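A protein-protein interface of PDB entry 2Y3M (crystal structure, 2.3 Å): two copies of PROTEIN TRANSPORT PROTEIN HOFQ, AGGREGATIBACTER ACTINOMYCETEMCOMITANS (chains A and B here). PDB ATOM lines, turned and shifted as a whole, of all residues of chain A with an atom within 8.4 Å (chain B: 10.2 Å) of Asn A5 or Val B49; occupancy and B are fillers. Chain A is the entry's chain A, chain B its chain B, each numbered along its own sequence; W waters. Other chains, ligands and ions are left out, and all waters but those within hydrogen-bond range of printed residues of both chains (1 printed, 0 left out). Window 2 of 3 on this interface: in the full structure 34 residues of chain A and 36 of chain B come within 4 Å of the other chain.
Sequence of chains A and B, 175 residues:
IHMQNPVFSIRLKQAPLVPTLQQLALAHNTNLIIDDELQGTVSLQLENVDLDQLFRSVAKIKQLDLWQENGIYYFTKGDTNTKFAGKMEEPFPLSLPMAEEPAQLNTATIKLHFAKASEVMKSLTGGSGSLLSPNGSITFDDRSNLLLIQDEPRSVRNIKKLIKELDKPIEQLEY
Among the printed residues, pairs that only touch across the chains: Asn A5 with Val B49 (3.5 Å), Pro A6 with Val B49 (3.6 Å), Val A7 with Asn B48 (3.7 Å), Phe A8 with Leu B46 (3.8 Å), Phe A8 with Glu B47 (3.3 Å), Phe A8 with Val B49 (3.6 Å), Phe A8 with Asp B50 (3.96 Å), Phe A8 with Leu B51 (3.6 Å), Phe A8 with Leu B54 (3.7 Å), Ser A9 with Leu B46 (3.2 Å), Ser A9 with Leu B54 (3.9 Å) and Lys A77 with Asn B31 (3.8 Å).
N of Phe A8 sits at hydrogen-bond distance from O of Asn B48 (2.8 Å).
The side-chain carboxylate of Glu B47 lies within salt-bridge range of the side-chain amino group of Lys A77 (3.0 Å).
Printed residues of chain A within 4 Å of Val B49: Asn A5 (3.5 Å), Pro A6 (3.6 Å) and Phe A8 (3.6 Å).
Phe A8 touches seven residues of chain B.
No residue of chain B comes within 4 Å of Thr A76.
Of the printed residues of chain B, Ser A9 touches Leu B46 (3.2 Å) and Leu B54 (3.9 Å).
Of the printed residues of chain B, Lys A77 touches Asn B31 and Glu B47.
Of the printed residues of chain A, Leu B51 touches Phe A8 (3.6 Å).
Asn B29 touches none of the printed residues of chain A.
Tyr A74 touches none of the printed residues of chain B.
The nearest residue of chain B that does not touch Asn A5 is Asn B48 (7.3 Å).
Of the 15 printed residues of chain A, 6 touch a printed residue of chain B.
Hydrophobic or aromatic side chains of chain A that line the printed part of chain B: Phe A8.
Among the printed residues, 14 pairs touch across the chains.
No position is printed for both chains.
N of Val A7 is in hydrogen-bond range of O of Phe A75.
ND2 of Asn B48 sits at hydrogen-bond distance from O of His B28 (2.7 Å).
The backbone carbonyl oxygen (O) of Asn B29 sits at hydrogen-bond distance from the side-chain amide nitrogen (ND2) of Asn B48, 3.3 Å away.
OG1 of Thr B30 lies within hydrogen-bond range of ND2 of Asn B48 (2.9 Å).
The backbone carbonyl oxygen (O) of Glu B47 lies within hydrogen-bond range of the backbone NH (N) of Asn B31, at 2.8 Å.
The side-chain amide oxygen (OD1) of Asn B48 sits at hydrogen-bond distance from the backbone NH (N) of Asp B50 (2.8 Å).
Water W1 bridges the backbone carbonyl oxygen of Pro A6 (2.7 Å) and the backbone carbonyl oxygen of Val B49 (2.9 Å).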
ATOM      1  N   GLN A   4      17.257 -26.038   5.982  1.00  0.00           N
ATOM      2  CA  GLN A   4      18.089 -24.798   5.982  1.00  0.00           C
ATOM      3  C   GLN A   4      19.197 -24.838   4.918  1.00  0.00           C
ATOM      4  O   GLN A   4      20.272 -24.264   5.106  1.00  0.00           O
ATOM      5  CB  GLN A   4      18.676 -24.543   7.378  1.00  0.00           C
ATOM      6  CG  GLN A   4      19.550 -25.669   7.927  1.00  0.00           C
ATOM      7  CD  GLN A   4      20.167 -25.326   9.269  1.00  0.00           C
ATOM      8  OE1 GLN A   4      19.463 -25.081  10.248  1.00  0.00           O
ATOM      9  NE2 GLN A   4      21.494 -25.315   9.323  1.00  0.00           N
ATOM     10  N   ASN A   5      18.918 -25.510   3.803  1.00  0.00           N
ATOM     11  CA  ASN A   5      19.888 -25.681   2.719  1.00  0.00           C
ATOM     12  C   ASN A   5      19.189 -25.878   1.366  1.00  0.00           C
ATOM     13  O   ASN A   5      18.460 -26.856   1.190  1.00  0.00           O
ATOM     14  CB  ASN A   5      20.816 -26.862   3.026  1.00  0.00           C
ATOM     15  CG  ASN A   5      22.052 -26.882   2.147  1.00  0.00           C
ATOM     16  OD1 ASN A   5      21.959 -26.905   0.919  1.00  0.00           O
ATOM     17  ND2 ASN A   5      23.223 -26.890   2.777  1.00  0.00           N
ATOM     18  N   PRO A   6      19.414 -24.950   0.408  1.00  0.00           N
ATOM     19  CA  PRO A   6      18.659 -24.917  -0.853  1.00  0.00           C
ATOM     20  C   PRO A   6      18.943 -26.086  -1.791  1.00  0.00           C
ATOM     21  O   PRO A   6      20.100 -26.478  -1.966  1.00  0.00           O
ATOM     22  CB  PRO A   6      19.086 -23.590  -1.493  1.00  0.00           C
ATOM     23  CG  PRO A   6      20.383 -23.255  -0.883  1.00  0.00           C
ATOM     24  CD  PRO A   6      20.395 -23.851   0.493  1.00  0.00           C
ATOM     25  N   VAL A   7      17.881 -26.635  -2.381  1.00  0.00           N
ATOM     26  CA  VAL A   7      17.990 -27.765  -3.304  1.00  0.00           C
ATOM     27  C   VAL A   7      17.251 -27.510  -4.607  1.00  0.00           C
ATOM     28  O   VAL A   7      16.237 -26.808  -4.631  1.00  0.00           O
ATOM     29  CB  VAL A   7      17.457 -29.106  -2.689  1.00  0.00           C
ATOM     30  CG1 VAL A   7      18.369 -29.614  -1.567  1.00  0.00           C
ATOM     31  CG2 VAL A   7      15.995 -28.982  -2.217  1.00  0.00           C
ATOM     32  N   PHE A   8      17.769 -28.084  -5.685  1.00  0.00           N
ATOM     33  CA  PHE A   8      17.018 -28.216  -6.926  1.00  0.00           C
ATOM     34  C   PHE A   8      16.247 -29.530  -6.880  1.00  0.00           C
ATOM     35  O   PHE A   8      16.791 -30.571  -6.490  1.00  0.00           O
ATOM     36  CB  PHE A   8      17.943 -28.183  -8.139  1.00  0.00           C
ATOM     37  CG  PHE A   8      18.625 -26.855  -8.344  1.00  0.00           C
ATOM     38  CD1 PHE A   8      18.020 -25.859  -9.107  1.00  0.00           C
ATOM     39  CD2 PHE A   8      19.874 -26.598  -7.763  1.00  0.00           C
ATOM     40  CE1 PHE A   8      18.644 -24.627  -9.299  1.00  0.00           C
ATOM     41  CE2 PHE A   8      20.506 -25.369  -7.950  1.00  0.00           C
ATOM     42  CZ  PHE A   8      19.895 -24.382  -8.721  1.00  0.00           C
ATOM     43  N   SER A   9      14.982 -29.471  -7.277  1.00  0.00           N
ATOM     44  CA  SER A   9      14.084 -30.612  -7.191  1.00  0.00           C
ATOM     45  C   SER A   9      13.391 -30.879  -8.519  1.00  0.00           C
ATOM     46  O   SER A   9      13.045 -29.950  -9.247  1.00  0.00           O
ATOM     47  CB  SER A   9      13.035 -30.367  -6.109  1.00  0.00           C
ATOM     48  OG  SER A   9      12.109 -31.432  -6.070  1.00  0.00           O
ATOM     49  N   TYR A  74      13.113 -24.965  -7.155  1.00  0.00           N
ATOM     50  CA  TYR A  74      14.279 -24.586  -6.351  1.00  0.00           C
ATOM     51  C   TYR A  74      13.790 -23.921  -5.070  1.00  0.00           C
ATOM     52  O   TYR A  74      13.169 -22.862  -5.113  1.00  0.00           O
ATOM     53  CB  TYR A  74      15.215 -23.670  -7.143  1.00  0.00           C
ATOM     54  CG  TYR A  74      16.368 -23.085  -6.340  1.00  0.00           C
ATOM     55  CD1 TYR A  74      17.519 -23.837  -6.077  1.00  0.00           C
ATOM     56  CD2 TYR A  74      16.311 -21.770  -5.862  1.00  0.00           C
ATOM     57  CE1 TYR A  74      18.589 -23.296  -5.343  1.00  0.00           C
ATOM     58  CE2 TYR A  74      17.372 -21.217  -5.129  1.00  0.00           C
ATOM     59  CZ  TYR A  74      18.509 -21.982  -4.874  1.00  0.00           C
ATOM     60  OH  TYR A  74      19.550 -21.431  -4.155  1.00  0.00           O
ATOM     61  N   PHE A  75      14.066 -24.558  -3.937  1.00  0.00           N
ATOM     62  CA  PHE A  75      13.477 -24.155  -2.663  1.00  0.00           C
ATOM     63  C   PHE A  75      14.347 -24.582  -1.491  1.00  0.00           C
ATOM     64  O   PHE A  75      15.378 -25.230  -1.679  1.00  0.00           O
ATOM     65  CB  PHE A  75      12.073 -24.757  -2.518  1.00  0.00           C
ATOM     66  CG  PHE A  75      12.065 -26.225  -2.174  1.00  0.00           C
ATOM     67  CD1 PHE A  75      12.441 -27.185  -3.115  1.00  0.00           C
ATOM     68  CD2 PHE A  75      11.656 -26.655  -0.910  1.00  0.00           C
ATOM     69  CE1 PHE A  75      12.421 -28.549  -2.796  1.00  0.00           C
ATOM     70  CE2 PHE A  75      11.631 -28.016  -0.584  1.00  0.00           C
ATOM     71  CZ  PHE A  75      12.016 -28.963  -1.531  1.00  0.00           C
ATOM     72  N   THR A  76      13.913 -24.224  -0.284  1.00  0.00           N
ATOM     73  CA  THR A  76      14.625 -24.584   0.938  1.00  0.00           C
ATOM     74  C   THR A  76      13.837 -25.609   1.748  1.00  0.00           C
ATOM     75  O   THR A  76      12.664 -25.401   2.064  1.00  0.00           O
ATOM     76  CB  THR A  76      14.938 -23.336   1.784  1.00  0.00           C
ATOM     77  OG1 THR A  76      15.741 -22.439   1.012  1.00  0.00           O
ATOM     78  CG2 THR A  76      15.699 -23.701   3.055  1.00  0.00           C
ATOM     79  N   LYS A  77      14.501 -26.719   2.066  1.00  0.00           N
ATOM     80  CA  LYS A  77      13.923 -27.789   2.875  1.00  0.00           C
ATOM     81  C   LYS A  77      13.695 -27.341   4.315  1.00  0.00           C
ATOM     82  O   LYS A  77      12.640 -26.803   4.646  1.00  0.00           O
ATOM     83  CB  LYS A  77      14.839 -29.011   2.862  1.00  0.00           C
ATOM     84  CG  LYS A  77      15.020 -29.654   1.491  1.00  0.00           C
ATOM     85  CD  LYS A  77      16.070 -30.763   1.526  1.00  0.00           C
ATOM     86  CE  LYS A  77      15.597 -31.985   2.312  1.00  0.00           C
ATOM     87  NZ  LYS A  77      14.425 -32.650   1.677  1.00  0.00           N
ATOM     88  N   THR A 125      22.432 -18.728  -8.487  1.00  0.00           N
ATOM     89  CA  THR A 125      22.635 -19.538  -7.282  1.00  0.00           C
ATOM     90  C   THR A 125      24.099 -19.920  -7.023  1.00  0.00           C
ATOM     91  O   THR A 125      24.381 -20.684  -6.102  1.00  0.00           O
ATOM     92  CB  THR A 125      21.787 -20.838  -7.321  1.00  0.00           C
ATOM     93  OG1 THR A 125      22.194 -21.643  -8.435  1.00  0.00           O
ATOM     94  CG2 THR A 125      20.298 -20.521  -7.439  1.00  0.00           C
ATOM     95  N   GLY A 127      27.747 -19.848  -5.556  1.00  0.00           N
ATOM     96  CA  GLY A 127      28.280 -19.429  -4.257  1.00  0.00           C
ATOM     97  C   GLY A 127      27.480 -19.884  -3.046  1.00  0.00           C
ATOM     98  O   GLY A 127      26.350 -20.372  -3.173  1.00  0.00           O
ATOM     99  N   SER A 128      28.072 -19.690  -1.869  1.00  0.00           N
ATOM    100  CA  SER A 128      27.538 -20.191  -0.592  1.00  0.00           C
ATOM    101  C   SER A 128      26.275 -19.497  -0.069  1.00  0.00           C
ATOM    102  O   SER A 128      25.435 -20.141   0.559  1.00  0.00           O
ATOM    103  CB  SER A 128      28.616 -20.111   0.487  1.00  0.00           C
ATOM    104  OG  SER A 128      29.773 -20.802   0.076  1.00  0.00           O
ATOM    105  N   SER A 130      22.598 -17.604   0.226  1.00  0.00           N
ATOM    106  CA  SER A 130      21.278 -17.932  -0.304  1.00  0.00           C
ATOM    107  C   SER A 130      20.785 -16.860  -1.268  1.00  0.00           C
ATOM    108  O   SER A 130      21.005 -15.670  -1.052  1.00  0.00           O
ATOM    109  CB  SER A 130      20.278 -18.094   0.838  1.00  0.00           C
ATOM    110  OG  SER A 130      20.700 -19.114   1.724  1.00  0.00           O
ATOM    111  N   PRO A 134      14.216 -17.943   3.402  1.00  0.00           N
ATOM    112  CA  PRO A 134      13.786 -19.307   3.723  1.00  0.00           C
ATOM    113  C   PRO A 134      12.448 -19.724   3.092  1.00  0.00           C
ATOM    114  O   PRO A 134      12.216 -20.921   2.873  1.00  0.00           O
ATOM    115  CB  PRO A 134      13.661 -19.278   5.248  1.00  0.00           C
ATOM    116  CG  PRO A 134      14.672 -18.274   5.675  1.00  0.00           C
ATOM    117  CD  PRO A 134      14.682 -17.217   4.603  1.00  0.00           C
ATOM    118  N   ALA B  25      20.887 -42.810  -6.782  1.00  0.00           N
ATOM    119  CA  ALA B  25      20.579 -41.507  -6.199  1.00  0.00           C
ATOM    120  C   ALA B  25      21.683 -41.101  -5.223  1.00  0.00           C
ATOM    121  O   ALA B  25      22.150 -39.961  -5.244  1.00  0.00           O
ATOM    122  CB  ALA B  25      19.224 -41.528  -5.501  1.00  0.00           C
ATOM    123  N   HIS B  28      25.172 -39.740  -6.739  1.00  0.00           N
ATOM    124  CA  HIS B  28      25.271 -38.341  -7.152  1.00  0.00           C
ATOM    125  C   HIS B  28      24.883 -37.387  -6.019  1.00  0.00           C
ATOM    126  O   HIS B  28      24.699 -36.189  -6.247  1.00  0.00           O
ATOM    127  CB  HIS B  28      24.425 -38.071  -8.403  1.00  0.00           C
ATOM    128  CG  HIS B  28      24.757 -38.960  -9.563  1.00  0.00           C
ATOM    129  ND1 HIS B  28      23.999 -40.064  -9.893  1.00  0.00           N
ATOM    130  CD2 HIS B  28      25.764 -38.911 -10.467  1.00  0.00           C
ATOM    131  CE1 HIS B  28      24.527 -40.656 -10.951  1.00  0.00           C
ATOM    132  NE2 HIS B  28      25.598 -39.975 -11.319  1.00  0.00           N
ATOM    133  N   ASN B  29      24.784 -37.922  -4.801  1.00  0.00           N
ATOM    134  CA  ASN B  29      24.361 -37.151  -3.632  1.00  0.00           C
ATOM    135  C   ASN B  29      22.960 -36.564  -3.842  1.00  0.00           C
ATOM    136  O   ASN B  29      22.682 -35.412  -3.498  1.00  0.00           O
ATOM    137  CB  ASN B  29      25.390 -36.054  -3.321  1.00  0.00           C
ATOM    138  CG  ASN B  29      25.405 -35.655  -1.860  1.00  0.00           C
ATOM    139  OD1 ASN B  29      25.063 -36.442  -0.976  1.00  0.00           O
ATOM    140  ND2 ASN B  29      25.826 -34.426  -1.598  1.00  0.00           N
ATOM    141  N   THR B  30      22.091 -37.375  -4.432  1.00  0.00           N
ATOM    142  CA  THR B  30      20.734 -36.978  -4.758  1.00  0.00           C
ATOM    143  C   THR B  30      19.771 -37.632  -3.781  1.00  0.00           C
ATOM    144  O   THR B  30      19.802 -38.845  -3.589  1.00  0.00           O
ATOM    145  CB  THR B  30      20.378 -37.379  -6.211  1.00  0.00           C
ATOM    146  OG1 THR B  30      21.163 -36.606  -7.123  1.00  0.00           O
ATOM    147  CG2 THR B  30      18.900 -37.156  -6.511  1.00  0.00           C
ATOM    148  N   ASN B  31      18.937 -36.820  -3.142  1.00  0.00           N
ATOM    149  CA  ASN B  31      17.854 -37.350  -2.320  1.00  0.00           C
ATOM    150  C   ASN B  31      16.720 -37.894  -3.204  1.00  0.00           C
ATOM    151  O   ASN B  31      16.373 -37.285  -4.219  1.00  0.00           O
ATOM    152  CB  ASN B  31      17.339 -36.289  -1.344  1.00  0.00           C
ATOM    153  CG  ASN B  31      16.376 -36.856  -0.315  1.00  0.00           C
ATOM    154  OD1 ASN B  31      16.437 -38.036   0.032  1.00  0.00           O
ATOM    155  ND2 ASN B  31      15.483 -36.011   0.182  1.00  0.00           N
ATOM    156  N   LEU B  46      13.318 -36.131  -7.028  1.00  0.00           N
ATOM    157  CA  LEU B  46      14.773 -36.091  -6.934  1.00  0.00           C
ATOM    158  C   LEU B  46      15.235 -34.731  -6.446  1.00  0.00           C
ATOM    159  O   LEU B  46      14.717 -33.701  -6.868  1.00  0.00           O
ATOM    160  CB  LEU B  46      15.406 -36.412  -8.286  1.00  0.00           C
ATOM    161  CG  LEU B  46      15.083 -37.803  -8.822  1.00  0.00           C
ATOM    162  CD1 LEU B  46      15.343 -37.854 -10.291  1.00  0.00           C
ATOM    163  CD2 LEU B  46      15.913 -38.841  -8.101  1.00  0.00           C
ATOM    164  N   GLU B  47      16.195 -34.738  -5.530  1.00  0.00           N
ATOM    165  CA  GLU B  47      16.713 -33.500  -4.964  1.00  0.00           C
ATOM    166  C   GLU B  47      18.227 -33.483  -4.976  1.00  0.00           C
ATOM    167  O   GLU B  47      18.864 -34.441  -4.554  1.00  0.00           O
ATOM    168  CB  GLU B  47      16.206 -33.312  -3.535  1.00  0.00           C
ATOM    169  CG  GLU B  47      14.732 -32.992  -3.439  1.00  0.00           C
ATOM    170  CD  GLU B  47      14.189 -33.163  -2.039  1.00  0.00           C
ATOM    171  OE1 GLU B  47      14.960 -33.522  -1.124  1.00  0.00           O
ATOM    172  OE2 GLU B  47      12.978 -32.938  -1.855  1.00  0.00           O
ATOM    173  N   ASN B  48      18.795 -32.386  -5.465  1.00  0.00           N
ATOM    174  CA  ASN B  48      20.238 -32.173  -5.387  1.00  0.00           C
ATOM    175  C   ASN B  48      20.576 -30.688  -5.208  1.00  0.00           C
ATOM    176  O   ASN B  48      19.935 -29.831  -5.810  1.00  0.00           O
ATOM    177  CB  ASN B  48      20.929 -32.754  -6.622  1.00  0.00           C
ATOM    178  CG  ASN B  48      22.396 -33.026  -6.397  1.00  0.00           C
ATOM    179  OD1 ASN B  48      23.172 -32.117  -6.093  1.00  0.00           O
ATOM    180  ND2 ASN B  48      22.795 -34.282  -6.557  1.00  0.00           N
ATOM    181  N   VAL B  49      21.579 -30.396  -4.376  1.00  0.00           N
ATOM    182  CA  VAL B  49      22.039 -29.011  -4.149  1.00  0.00           C
ATOM    183  C   VAL B  49      22.647 -28.411  -5.421  1.00  0.00           C
ATOM    184  O   VAL B  49      22.645 -27.192  -5.603  1.00  0.00           O
ATOM    185  CB  VAL B  49      23.036 -28.883  -2.947  1.00  0.00           C
ATOM    186  CG1 VAL B  49      22.368 -29.261  -1.634  1.00  0.00           C
ATOM    187  CG2 VAL B  49      24.296 -29.712  -3.167  1.00  0.00           C
ATOM    188  N   ASP B  50      23.153 -29.281  -6.294  1.00  0.00           N
ATOM    189  CA  ASP B  50      23.669 -28.883  -7.604  1.00  0.00           C
ATOM    190  C   ASP B  50      22.671 -29.238  -8.698  1.00  0.00           C
ATOM    191  O   ASP B  50      22.128 -30.349  -8.714  1.00  0.00           O
ATOM    192  CB  ASP B  50      25.004 -29.577  -7.896  1.00  0.00           C
ATOM    193  CG  ASP B  50      26.195 -28.850  -7.288  1.00  0.00           C
ATOM    194  OD1 ASP B  50      26.306 -27.616  -7.450  1.00  0.00           O
ATOM    195  OD2 ASP B  50      27.041 -29.519  -6.662  1.00  0.00           O
ATOM    196  N   LEU B  51      22.438 -28.293  -9.604  1.00  0.00           N
ATOM    197  CA  LEU B  51      21.557 -28.516 -10.748  1.00  0.00           C
ATOM    198  C   LEU B  51      22.106 -29.537 -11.758  1.00  0.00           C
ATOM    199  O   LEU B  51      21.360 -30.390 -12.236  1.00  0.00           O
ATOM    200  CB  LEU B  51      21.226 -27.194 -11.455  1.00  0.00           C
ATOM    201  CG  LEU B  51      20.204 -27.249 -12.603  1.00  0.00           C
ATOM    202  CD1 LEU B  51      18.906 -27.928 -12.171  1.00  0.00           C
ATOM    203  CD2 LEU B  51      19.925 -25.858 -13.161  1.00  0.00           C
ATOM    204  N   ASP B  52      23.392 -29.437 -12.088  1.00  0.00           N
ATOM    205  CA  ASP B  52      24.007 -30.336 -13.071  1.00  0.00           C
ATOM    206  C   ASP B  52      24.000 -31.781 -12.570  1.00  0.00           C
ATOM    207  O   ASP B  52      23.851 -32.720 -13.350  1.00  0.00           O
ATOM    208  CB  ASP B  52      25.435 -29.888 -13.423  1.00  0.00           C
ATOM    209  CG  ASP B  52      26.394 -29.962 -12.230  1.00  0.00           C
ATOM    210  OD1 ASP B  52      25.939 -29.856 -11.067  1.00  0.00           O
ATOM    211  OD2 ASP B  52      27.612 -30.120 -12.454  1.00  0.00           O
ATOM    212  N   GLN B  53      24.151 -31.938 -11.260  1.00  0.00           N
ATOM    213  CA  GLN B  53      24.157 -33.241 -10.622  1.00  0.00           C
ATOM    214  C   GLN B  53      22.745 -33.833 -10.606  1.00  0.00           C
ATOM    215  O   GLN B  53      22.575 -35.041 -10.762  1.00  0.00           O
ATOM    216  CB  GLN B  53      24.745 -33.142  -9.212  1.00  0.00           C
ATOM    217  CG  GLN B  53      25.498 -34.384  -8.754  1.00  0.00           C
ATOM    218  CD  GLN B  53      26.878 -34.537  -9.381  1.00  0.00           C
ATOM    219  OE1 GLN B  53      27.312 -33.706 -10.179  1.00  0.00           O
ATOM    220  NE2 GLN B  53      27.578 -35.603  -9.007  1.00  0.00           N
ATOM    221  N   LEU B  54      21.742 -32.971 -10.445  1.00  0.00           N
ATOM    222  CA  LEU B  54      20.344 -33.381 -10.565  1.00  0.00           C
ATOM    223  C   LEU B  54      20.039 -33.912 -11.979  1.00  0.00           C
ATOM    224  O   LEU B  54      19.439 -34.981 -12.116  1.00  0.00           O
ATOM    225  CB  LEU B  54      19.392 -32.236 -10.194  1.00  0.00           C
ATOM    226  CG  LEU B  54      17.877 -32.518 -10.217  1.00  0.00           C
ATOM    227  CD1 LEU B  54      17.462 -33.482  -9.106  1.00  0.00           C
ATOM    228  CD2 LEU B  54      17.078 -31.229 -10.118  1.00  0.00           C
ATOM    229  N   PHE B  55      20.468 -33.176 -13.011  1.00  0.00           N
ATOM    230  CA  PHE B  55      20.269 -33.578 -14.406  1.00  0.00           C
ATOM    231  C   PHE B  55      20.874 -34.948 -14.701  1.00  0.00           C
ATOM    232  O   PHE B  55      20.274 -35.762 -15.415  1.00  0.00           O
ATOM    233  CB  PHE B  55      20.859 -32.553 -15.382  1.00  0.00           C
ATOM    234  CG  PHE B  55      20.037 -31.295 -15.541  1.00  0.00           C
ATOM    235  CD1 PHE B  55      18.645 -31.327 -15.479  1.00  0.00           C
ATOM    236  CD2 PHE B  55      20.665 -30.078 -15.795  1.00  0.00           C
ATOM    237  CE1 PHE B  55      17.894 -30.161 -15.640  1.00  0.00           C
ATOM    238  CE2 PHE B  55      19.924 -28.911 -15.962  1.00  0.00           C
ATOM    239  CZ  PHE B  55      18.536 -28.952 -15.883  1.00  0.00           C
ATOM    240  N   SER B  57      21.447 -37.343 -12.498  1.00  0.00           N
ATOM    241  CA  SER B  57      20.605 -38.315 -11.809  1.00  0.00           C
ATOM    242  C   SER B  57      19.398 -38.665 -12.666  1.00  0.00           C
ATOM    243  O   SER B  57      19.031 -39.829 -12.768  1.00  0.00           O
ATOM    244  CB  SER B  57      20.140 -37.780 -10.450  1.00  0.00           C
ATOM    245  OG  SER B  57      21.174 -37.835  -9.488  1.00  0.00           O
HETATM  246  O   HOH W   1      21.902 -25.201  -3.596  1.00  0.00           O
